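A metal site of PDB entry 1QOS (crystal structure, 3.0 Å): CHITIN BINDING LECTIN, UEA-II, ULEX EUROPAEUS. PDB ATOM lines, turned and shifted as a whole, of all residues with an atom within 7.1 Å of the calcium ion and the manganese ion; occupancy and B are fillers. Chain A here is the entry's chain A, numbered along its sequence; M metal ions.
The manganese ion is bound by OD1 of Asp 139 (1.9 Å), OE2 of Glu 126 (1.9 Å), OD2 of Asp 128 (2.1 Å) and NE2 of His 144 (2.2 Å).
The manganese ion has four donor atoms within binding distance.
The side-chain carboxylate (OD2) of Asp 148 sits close to the side-chain carboxylate (OE1) of Glu 126 (2.6 Å).
OD1 of Asp 139 lies close to NE1 of Trp 138.
The side-chain carboxylate (OD1) of Asp 148 is in hydrogen-bond range of the side-chain hydroxyl (OG) of Ser 154 (2.7 Å).
The backbone NH (N) of Tyr 130 sits at hydrogen-bond distance from the backbone carbonyl oxygen (O) of Asp 86 (3.4 Å).
The side-chain carboxylate (OE2) of Glu 126 sits close to the side-chain hydroxyl (OG) of Ser 154.
The backbone carbonyl oxygen (O) of Gly 146 is in hydrogen-bond range of the backbone NH (N) of Glu 126.
The backbone carbonyl oxygen of Gly 132 sits at hydrogen-bond distance from the side-chain hydroxyl of Tyr 130, 3.2 Å away.
ND1 of His 144 lies within hydrogen-bond range of O of Phe 142 (2.8 Å).
Residues that only touch the manganese ion: Ser 154.
Of the 26 residues printed, 5 come within 4 Å of the manganese ion.
Along chain A the residues within 4 Å of the manganese ion span positions 126 to 154.
The calcium ion is bound by the side-chain carboxylate (OD1) of Asp 128, the side-chain amide oxygen (OD1) of Asn 136, the side-chain carboxylate (OD2) of Asp 139 and the backbone carbonyl oxygen (O) of Tyr 130.
The calcium ion has four donor atoms within binding distance.
Slightly farther from the calcium ion lies the side-chain carboxylate (OD2) of Asp 128 (2.9 Å).
Within 4 Å of the calcium ion: Asp 128, Tyr 130, Asn 136 and Asp 139.
The nearest printed residue that does not touch the calcium ion is Asp 86 (4.4 Å).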
ATOM      1  N   ASP A  86      29.576  -7.772 -20.932  1.00  0.00           N
ATOM      2  CA  ASP A  86      28.522  -8.772 -21.086  1.00  0.00           C
ATOM      3  C   ASP A  86      28.008  -9.287 -19.758  1.00  0.00           C
ATOM      4  O   ASP A  86      26.903  -9.851 -19.687  1.00  0.00           O
ATOM      5  CB  ASP A  86      29.046  -9.984 -21.860  1.00  0.00           C
ATOM      6  CG  ASP A  86      28.779  -9.897 -23.331  1.00  0.00           C
ATOM      7  OD1 ASP A  86      27.615 -10.099 -23.738  1.00  0.00           O
ATOM      8  OD2 ASP A  86      29.737  -9.619 -24.081  1.00  0.00           O
ATOM      9  N   GLY A  87      28.849  -9.169 -18.736  1.00  0.00           N
ATOM     10  CA  GLY A  87      28.489  -9.648 -17.418  1.00  0.00           C
ATOM     11  C   GLY A  87      29.649 -10.166 -16.606  1.00  0.00           C
ATOM     12  O   GLY A  87      30.776 -10.331 -17.081  1.00  0.00           O
ATOM     13  N   ALA A 105      32.466 -13.995 -24.736  1.00  0.00           N
ATOM     14  CA  ALA A 105      32.037 -13.110 -23.672  1.00  0.00           C
ATOM     15  C   ALA A 105      30.677 -13.512 -23.071  1.00  0.00           C
ATOM     16  O   ALA A 105      30.504 -13.469 -21.852  1.00  0.00           O
ATOM     17  CB  ALA A 105      31.978 -11.706 -24.181  1.00  0.00           C
ATOM     18  N   GLY A 106      29.736 -13.931 -23.911  1.00  0.00           N
ATOM     19  CA  GLY A 106      28.430 -14.331 -23.418  1.00  0.00           C
ATOM     20  C   GLY A 106      28.440 -15.594 -22.585  1.00  0.00           C
ATOM     21  O   GLY A 106      27.440 -15.918 -21.939  1.00  0.00           O
ATOM     22  N   MET A 107      29.549 -16.330 -22.617  1.00  0.00           N
ATOM     23  CA  MET A 107      29.677 -17.580 -21.849  1.00  0.00           C
ATOM     24  C   MET A 107      30.672 -17.383 -20.697  1.00  0.00           C
ATOM     25  O   MET A 107      31.158 -18.343 -20.082  1.00  0.00           O
ATOM     26  CB  MET A 107      30.065 -18.739 -22.779  1.00  0.00           C
ATOM     27  CG  MET A 107      29.093 -18.925 -23.955  1.00  0.00           C
ATOM     28  SD  MET A 107      29.433 -20.278 -25.115  1.00  0.00           S
ATOM     29  CE  MET A 107      31.038 -19.775 -25.820  1.00  0.00           C
ATOM     30  N   PHE A 108      30.959 -16.117 -20.417  1.00  0.00           N
ATOM     31  CA  PHE A 108      31.858 -15.675 -19.351  1.00  0.00           C
ATOM     32  C   PHE A 108      33.141 -16.465 -19.191  1.00  0.00           C
ATOM     33  O   PHE A 108      33.701 -16.502 -18.099  1.00  0.00           O
ATOM     34  CB  PHE A 108      31.094 -15.620 -18.040  1.00  0.00           C
ATOM     35  CG  PHE A 108      29.765 -14.959 -18.149  1.00  0.00           C
ATOM     36  CD1 PHE A 108      29.660 -13.589 -18.359  1.00  0.00           C
ATOM     37  CD2 PHE A 108      28.592 -15.700 -18.065  1.00  0.00           C
ATOM     38  CE1 PHE A 108      28.424 -12.966 -18.479  1.00  0.00           C
ATOM     39  CE2 PHE A 108      27.348 -15.095 -18.183  1.00  0.00           C
ATOM     40  CZ  PHE A 108      27.256 -13.720 -18.395  1.00  0.00           C
ATOM     41  N   GLU A 126      25.844 -15.980 -12.319  1.00  0.00           N
ATOM     42  CA  GLU A 126      26.079 -14.954 -13.316  1.00  0.00           C
ATOM     43  C   GLU A 126      25.338 -13.654 -13.053  1.00  0.00           C
ATOM     44  O   GLU A 126      24.232 -13.644 -12.515  1.00  0.00           O
ATOM     45  CB  GLU A 126      25.722 -15.462 -14.718  1.00  0.00           C
ATOM     46  CG  GLU A 126      24.256 -15.830 -14.901  1.00  0.00           C
ATOM     47  CD  GLU A 126      23.884 -16.120 -16.349  1.00  0.00           C
ATOM     48  OE1 GLU A 126      24.692 -16.740 -17.084  1.00  0.00           O
ATOM     49  OE2 GLU A 126      22.776 -15.719 -16.760  1.00  0.00           O
ATOM     50  N   PHE A 127      25.995 -12.575 -13.448  1.00  0.00           N
ATOM     51  CA  PHE A 127      25.478 -11.213 -13.345  1.00  0.00           C
ATOM     52  C   PHE A 127      25.508 -10.713 -14.785  1.00  0.00           C
ATOM     53  O   PHE A 127      26.400  -9.971 -15.168  1.00  0.00           O
ATOM     54  CB  PHE A 127      26.360 -10.390 -12.439  1.00  0.00           C
ATOM     55  CG  PHE A 127      26.393 -10.885 -11.037  1.00  0.00           C
ATOM     56  CD1 PHE A 127      25.418 -10.488 -10.124  1.00  0.00           C
ATOM     57  CD2 PHE A 127      27.377 -11.786 -10.626  1.00  0.00           C
ATOM     58  CE1 PHE A 127      25.416 -10.989  -8.819  1.00  0.00           C
ATOM     59  CE2 PHE A 127      27.388 -12.281  -9.323  1.00  0.00           C
ATOM     60  CZ  PHE A 127      26.403 -11.881  -8.418  1.00  0.00           C
ATOM     61  N   ASP A 128      24.558 -11.230 -15.550  1.00  0.00           N
ATOM     62  CA  ASP A 128      24.366 -10.965 -16.976  1.00  0.00           C
ATOM     63  C   ASP A 128      23.868  -9.555 -17.270  1.00  0.00           C
ATOM     64  O   ASP A 128      22.766  -9.210 -16.833  1.00  0.00           O
ATOM     65  CB  ASP A 128      23.335 -11.969 -17.495  1.00  0.00           C
ATOM     66  CG  ASP A 128      23.748 -12.640 -18.785  1.00  0.00           C
ATOM     67  OD1 ASP A 128      24.308 -11.946 -19.651  1.00  0.00           O
ATOM     68  OD2 ASP A 128      23.493 -13.864 -18.929  1.00  0.00           O
ATOM     69  N   THR A 129      24.635  -8.760 -18.002  1.00  0.00           N
ATOM     70  CA  THR A 129      24.230  -7.393 -18.367  1.00  0.00           C
ATOM     71  C   THR A 129      23.669  -7.349 -19.791  1.00  0.00           C
ATOM     72  O   THR A 129      22.936  -6.425 -20.163  1.00  0.00           O
ATOM     73  CB  THR A 129      25.393  -6.390 -18.317  1.00  0.00           C
ATOM     74  OG1 THR A 129      26.515  -6.936 -19.022  1.00  0.00           O
ATOM     75  CG2 THR A 129      25.784  -6.099 -16.902  1.00  0.00           C
ATOM     76  N   TYR A 130      24.041  -8.341 -20.583  1.00  0.00           N
ATOM     77  CA  TYR A 130      23.577  -8.449 -21.954  1.00  0.00           C
ATOM     78  C   TYR A 130      22.632  -9.633 -22.126  1.00  0.00           C
ATOM     79  O   TYR A 130      22.997 -10.776 -21.844  1.00  0.00           O
ATOM     80  CB  TYR A 130      24.750  -8.583 -22.910  1.00  0.00           C
ATOM     81  CG  TYR A 130      24.309  -8.811 -24.320  1.00  0.00           C
ATOM     82  CD1 TYR A 130      23.805  -7.771 -25.097  1.00  0.00           C
ATOM     83  CD2 TYR A 130      24.324 -10.087 -24.869  1.00  0.00           C
ATOM     84  CE1 TYR A 130      23.316  -7.992 -26.381  1.00  0.00           C
ATOM     85  CE2 TYR A 130      23.850 -10.324 -26.154  1.00  0.00           C
ATOM     86  CZ  TYR A 130      23.341  -9.279 -26.899  1.00  0.00           C
ATOM     87  OH  TYR A 130      22.840  -9.506 -28.172  1.00  0.00           O
ATOM     88  N   PHE A 131      21.466  -9.362 -22.687  1.00  0.00           N
ATOM     89  CA  PHE A 131      20.436 -10.374 -22.874  1.00  0.00           C
ATOM     90  C   PHE A 131      19.811 -10.420 -24.258  1.00  0.00           C
ATOM     91  O   PHE A 131      18.795 -11.094 -24.456  1.00  0.00           O
ATOM     92  CB  PHE A 131      19.331 -10.143 -21.849  1.00  0.00           C
ATOM     93  CG  PHE A 131      18.737  -8.765 -21.919  1.00  0.00           C
ATOM     94  CD1 PHE A 131      19.445  -7.660 -21.454  1.00  0.00           C
ATOM     95  CD2 PHE A 131      17.462  -8.565 -22.425  1.00  0.00           C
ATOM     96  CE1 PHE A 131      18.902  -6.376 -21.507  1.00  0.00           C
ATOM     97  CE2 PHE A 131      16.901  -7.296 -22.485  1.00  0.00           C
ATOM     98  CZ  PHE A 131      17.618  -6.195 -22.021  1.00  0.00           C
ATOM     99  N   GLY A 132      20.407  -9.693 -25.209  1.00  0.00           N
ATOM    100  CA  GLY A 132      19.903  -9.657 -26.580  1.00  0.00           C
ATOM    101  C   GLY A 132      19.816 -11.029 -27.223  1.00  0.00           C
ATOM    102  O   GLY A 132      20.778 -11.791 -27.217  1.00  0.00           O
ATOM    103  N   ASN A 136      22.520 -13.971 -27.686  1.00  0.00           N
ATOM    104  CA  ASN A 136      22.292 -14.699 -26.427  1.00  0.00           C
ATOM    105  C   ASN A 136      20.828 -15.126 -26.387  1.00  0.00           C
ATOM    106  O   ASN A 136      20.031 -14.563 -25.642  1.00  0.00           O
ATOM    107  CB  ASN A 136      22.557 -13.803 -25.207  1.00  0.00           C
ATOM    108  CG  ASN A 136      24.026 -13.661 -24.856  1.00  0.00           C
ATOM    109  OD1 ASN A 136      24.358 -13.242 -23.750  1.00  0.00           O
ATOM    110  ND2 ASN A 136      24.916 -13.994 -25.791  1.00  0.00           N
ATOM    111  N   TRP A 138      19.365 -17.761 -25.122  1.00  0.00           N
ATOM    112  CA  TRP A 138      18.976 -18.427 -23.885  1.00  0.00           C
ATOM    113  C   TRP A 138      18.511 -17.482 -22.778  1.00  0.00           C
ATOM    114  O   TRP A 138      17.652 -17.849 -21.977  1.00  0.00           O
ATOM    115  CB  TRP A 138      20.148 -19.242 -23.359  1.00  0.00           C
ATOM    116  CG  TRP A 138      21.407 -18.445 -23.264  1.00  0.00           C
ATOM    117  CD1 TRP A 138      21.730 -17.549 -22.292  1.00  0.00           C
ATOM    118  CD2 TRP A 138      22.491 -18.424 -24.203  1.00  0.00           C
ATOM    119  NE1 TRP A 138      22.940 -16.965 -22.558  1.00  0.00           N
ATOM    120  CE2 TRP A 138      23.437 -17.486 -23.722  1.00  0.00           C
ATOM    121  CE3 TRP A 138      22.759 -19.106 -25.394  1.00  0.00           C
ATOM    122  CZ2 TRP A 138      24.641 -17.212 -24.401  1.00  0.00           C
ATOM    123  CZ3 TRP A 138      23.950 -18.837 -26.072  1.00  0.00           C
ATOM    124  CH2 TRP A 138      24.880 -17.891 -25.569  1.00  0.00           C
ATOM    125  N   ASP A 139      19.082 -16.281 -22.733  1.00  0.00           N
ATOM    126  CA  ASP A 139      18.759 -15.280 -21.716  1.00  0.00           C
ATOM    127  C   ASP A 139      17.331 -14.740 -21.800  1.00  0.00           C
ATOM    128  O   ASP A 139      16.725 -14.716 -22.875  1.00  0.00           O
ATOM    129  CB  ASP A 139      19.744 -14.088 -21.801  1.00  0.00           C
ATOM    130  CG  ASP A 139      21.126 -14.398 -21.204  1.00  0.00           C
ATOM    131  OD1 ASP A 139      21.229 -15.215 -20.255  1.00  0.00           O
ATOM    132  OD2 ASP A 139      22.109 -13.784 -21.665  1.00  0.00           O
ATOM    133  N   PRO A 140      16.774 -14.337 -20.655  1.00  0.00           N
ATOM    134  CA  PRO A 140      15.426 -13.750 -20.569  1.00  0.00           C
ATOM    135  C   PRO A 140      15.438 -12.308 -21.067  1.00  0.00           C
ATOM    136  O   PRO A 140      16.483 -11.778 -21.453  1.00  0.00           O
ATOM    137  CB  PRO A 140      15.130 -13.820 -19.070  1.00  0.00           C
ATOM    138  CG  PRO A 140      16.463 -13.658 -18.461  1.00  0.00           C
ATOM    139  CD  PRO A 140      17.315 -14.572 -19.303  1.00  0.00           C
ATOM    140  N   PHE A 142      15.672  -9.368 -19.854  1.00  0.00           N
ATOM    141  CA  PHE A 142      16.183  -8.335 -18.950  1.00  0.00           C
ATOM    142  C   PHE A 142      17.537  -8.664 -18.339  1.00  0.00           C
ATOM    143  O   PHE A 142      18.003  -9.810 -18.412  1.00  0.00           O
ATOM    144  CB  PHE A 142      15.170  -8.036 -17.837  1.00  0.00           C
ATOM    145  CG  PHE A 142      14.576  -9.262 -17.214  1.00  0.00           C
ATOM    146  CD1 PHE A 142      15.390 -10.285 -16.728  1.00  0.00           C
ATOM    147  CD2 PHE A 142      13.212  -9.400 -17.114  1.00  0.00           C
ATOM    148  CE1 PHE A 142      14.842 -11.437 -16.163  1.00  0.00           C
ATOM    149  CE2 PHE A 142      12.653 -10.549 -16.558  1.00  0.00           C
ATOM    150  CZ  PHE A 142      13.470 -11.563 -16.083  1.00  0.00           C
ATOM    151  N   HIS A 144      19.874  -9.801 -15.697  1.00  0.00           N
ATOM    152  CA  HIS A 144      19.552 -10.758 -14.662  1.00  0.00           C
ATOM    153  C   HIS A 144      20.709 -11.317 -13.828  1.00  0.00           C
ATOM    154  O   HIS A 144      21.884 -11.132 -14.139  1.00  0.00           O
ATOM    155  CB  HIS A 144      18.826 -11.936 -15.324  1.00  0.00           C
ATOM    156  CG  HIS A 144      19.598 -12.562 -16.457  1.00  0.00           C
ATOM    157  ND1 HIS A 144      19.637 -12.008 -17.718  1.00  0.00           N
ATOM    158  CD2 HIS A 144      20.358 -13.681 -16.516  1.00  0.00           C
ATOM    159  CE1 HIS A 144      20.386 -12.760 -18.513  1.00  0.00           C
ATOM    160  NE2 HIS A 144      20.834 -13.784 -17.811  1.00  0.00           N
ATOM    161  N   ILE A 145      20.327 -11.977 -12.744  1.00  0.00           N
ATOM    162  CA  ILE A 145      21.250 -12.699 -11.867  1.00  0.00           C
ATOM    163  C   ILE A 145      20.796 -14.115 -12.142  1.00  0.00           C
ATOM    164  O   ILE A 145      19.580 -14.394 -12.147  1.00  0.00           O
ATOM    165  CB  ILE A 145      20.983 -12.425 -10.371  1.00  0.00           C
ATOM    166  CG1 ILE A 145      21.356 -10.993 -10.006  1.00  0.00           C
ATOM    167  CG2 ILE A 145      21.787 -13.383  -9.524  1.00  0.00           C
ATOM    168  CD1 ILE A 145      21.149 -10.691  -8.549  1.00  0.00           C
ATOM    169  N   GLY A 146      21.727 -15.016 -12.410  1.00  0.00           N
ATOM    170  CA  GLY A 146      21.328 -16.377 -12.683  1.00  0.00           C
ATOM    171  C   GLY A 146      22.216 -17.440 -12.074  1.00  0.00           C
ATOM    172  O   GLY A 146      23.409 -17.221 -11.854  1.00  0.00           O
ATOM    173  N   ASP A 148      23.796 -20.872 -12.718  1.00  0.00           N
ATOM    174  CA  ASP A 148      24.119 -21.701 -13.862  1.00  0.00           C
ATOM    175  C   ASP A 148      24.677 -23.025 -13.426  1.00  0.00           C
ATOM    176  O   ASP A 148      25.622 -23.074 -12.633  1.00  0.00           O
ATOM    177  CB  ASP A 148      25.140 -21.007 -14.763  1.00  0.00           C
ATOM    178  CG  ASP A 148      24.632 -19.688 -15.305  1.00  0.00           C
ATOM    179  OD1 ASP A 148      23.409 -19.447 -15.294  1.00  0.00           O
ATOM    180  OD2 ASP A 148      25.481 -18.880 -15.735  1.00  0.00           O
ATOM    181  N   ILE A 152      25.130 -22.503 -19.665  1.00  0.00           N
ATOM    182  CA  ILE A 152      24.967 -21.048 -19.629  1.00  0.00           C
ATOM    183  C   ILE A 152      23.477 -20.646 -19.580  1.00  0.00           C
ATOM    184  O   ILE A 152      23.138 -19.473 -19.342  1.00  0.00           O
ATOM    185  CB  ILE A 152      25.679 -20.397 -20.834  1.00  0.00           C
ATOM    186  CG1 ILE A 152      25.751 -18.882 -20.646  1.00  0.00           C
ATOM    187  CG2 ILE A 152      24.986 -20.775 -22.119  1.00  0.00           C
ATOM    188  CD1 ILE A 152      26.662 -18.429 -19.521  1.00  0.00           C
ATOM    189  N   LYS A 153      22.590 -21.610 -19.826  1.00  0.00           N
ATOM    190  CA  LYS A 153      21.154 -21.378 -19.748  1.00  0.00           C
ATOM    191  C   LYS A 153      20.811 -21.614 -18.278  1.00  0.00           C
ATOM    192  O   LYS A 153      20.678 -22.753 -17.815  1.00  0.00           O
ATOM    193  CB  LYS A 153      20.387 -22.344 -20.664  1.00  0.00           C
ATOM    194  CG  LYS A 153      18.885 -22.075 -20.731  1.00  0.00           C
ATOM    195  CD  LYS A 153      18.198 -22.872 -21.832  1.00  0.00           C
ATOM    196  CE  LYS A 153      16.675 -22.684 -21.793  1.00  0.00           C
ATOM    197  NZ  LYS A 153      16.267 -21.234 -21.807  1.00  0.00           N
ATOM    198  N   SER A 154      20.755 -20.522 -17.528  1.00  0.00           N
ATOM    199  CA  SER A 154      20.470 -20.547 -16.092  1.00  0.00           C
ATOM    200  C   SER A 154      19.270 -21.421 -15.768  1.00  0.00           C
ATOM    201  O   SER A 154      18.346 -21.510 -16.570  1.00  0.00           O
ATOM    202  CB  SER A 154      20.213 -19.136 -15.569  1.00  0.00           C
ATOM    203  OG  SER A 154      21.120 -18.199 -16.131  1.00  0.00           O
ATOM    204  N   THR A 157      16.520 -17.608 -12.776  1.00  0.00           N
ATOM    205  CA  THR A 157      17.003 -16.233 -12.876  1.00  0.00           C
ATOM    206  C   THR A 157      16.059 -15.302 -12.144  1.00  0.00           C
ATOM    207  O   THR A 157      14.985 -15.699 -11.709  1.00  0.00           O
ATOM    208  CB  THR A 157      17.089 -15.746 -14.352  1.00  0.00           C
ATOM    209  OG1 THR A 157      15.833 -15.974 -15.009  1.00  0.00           O
ATOM    210  CG2 THR A 157      18.186 -16.480 -15.099  1.00  0.00           C
HETATM  211 CA    CA M   1      24.191 -12.801 -21.556  1.00  0.00          CA
HETATM  212 MN    MN M   2      22.105 -15.414 -18.552  1.00  0.00          MN
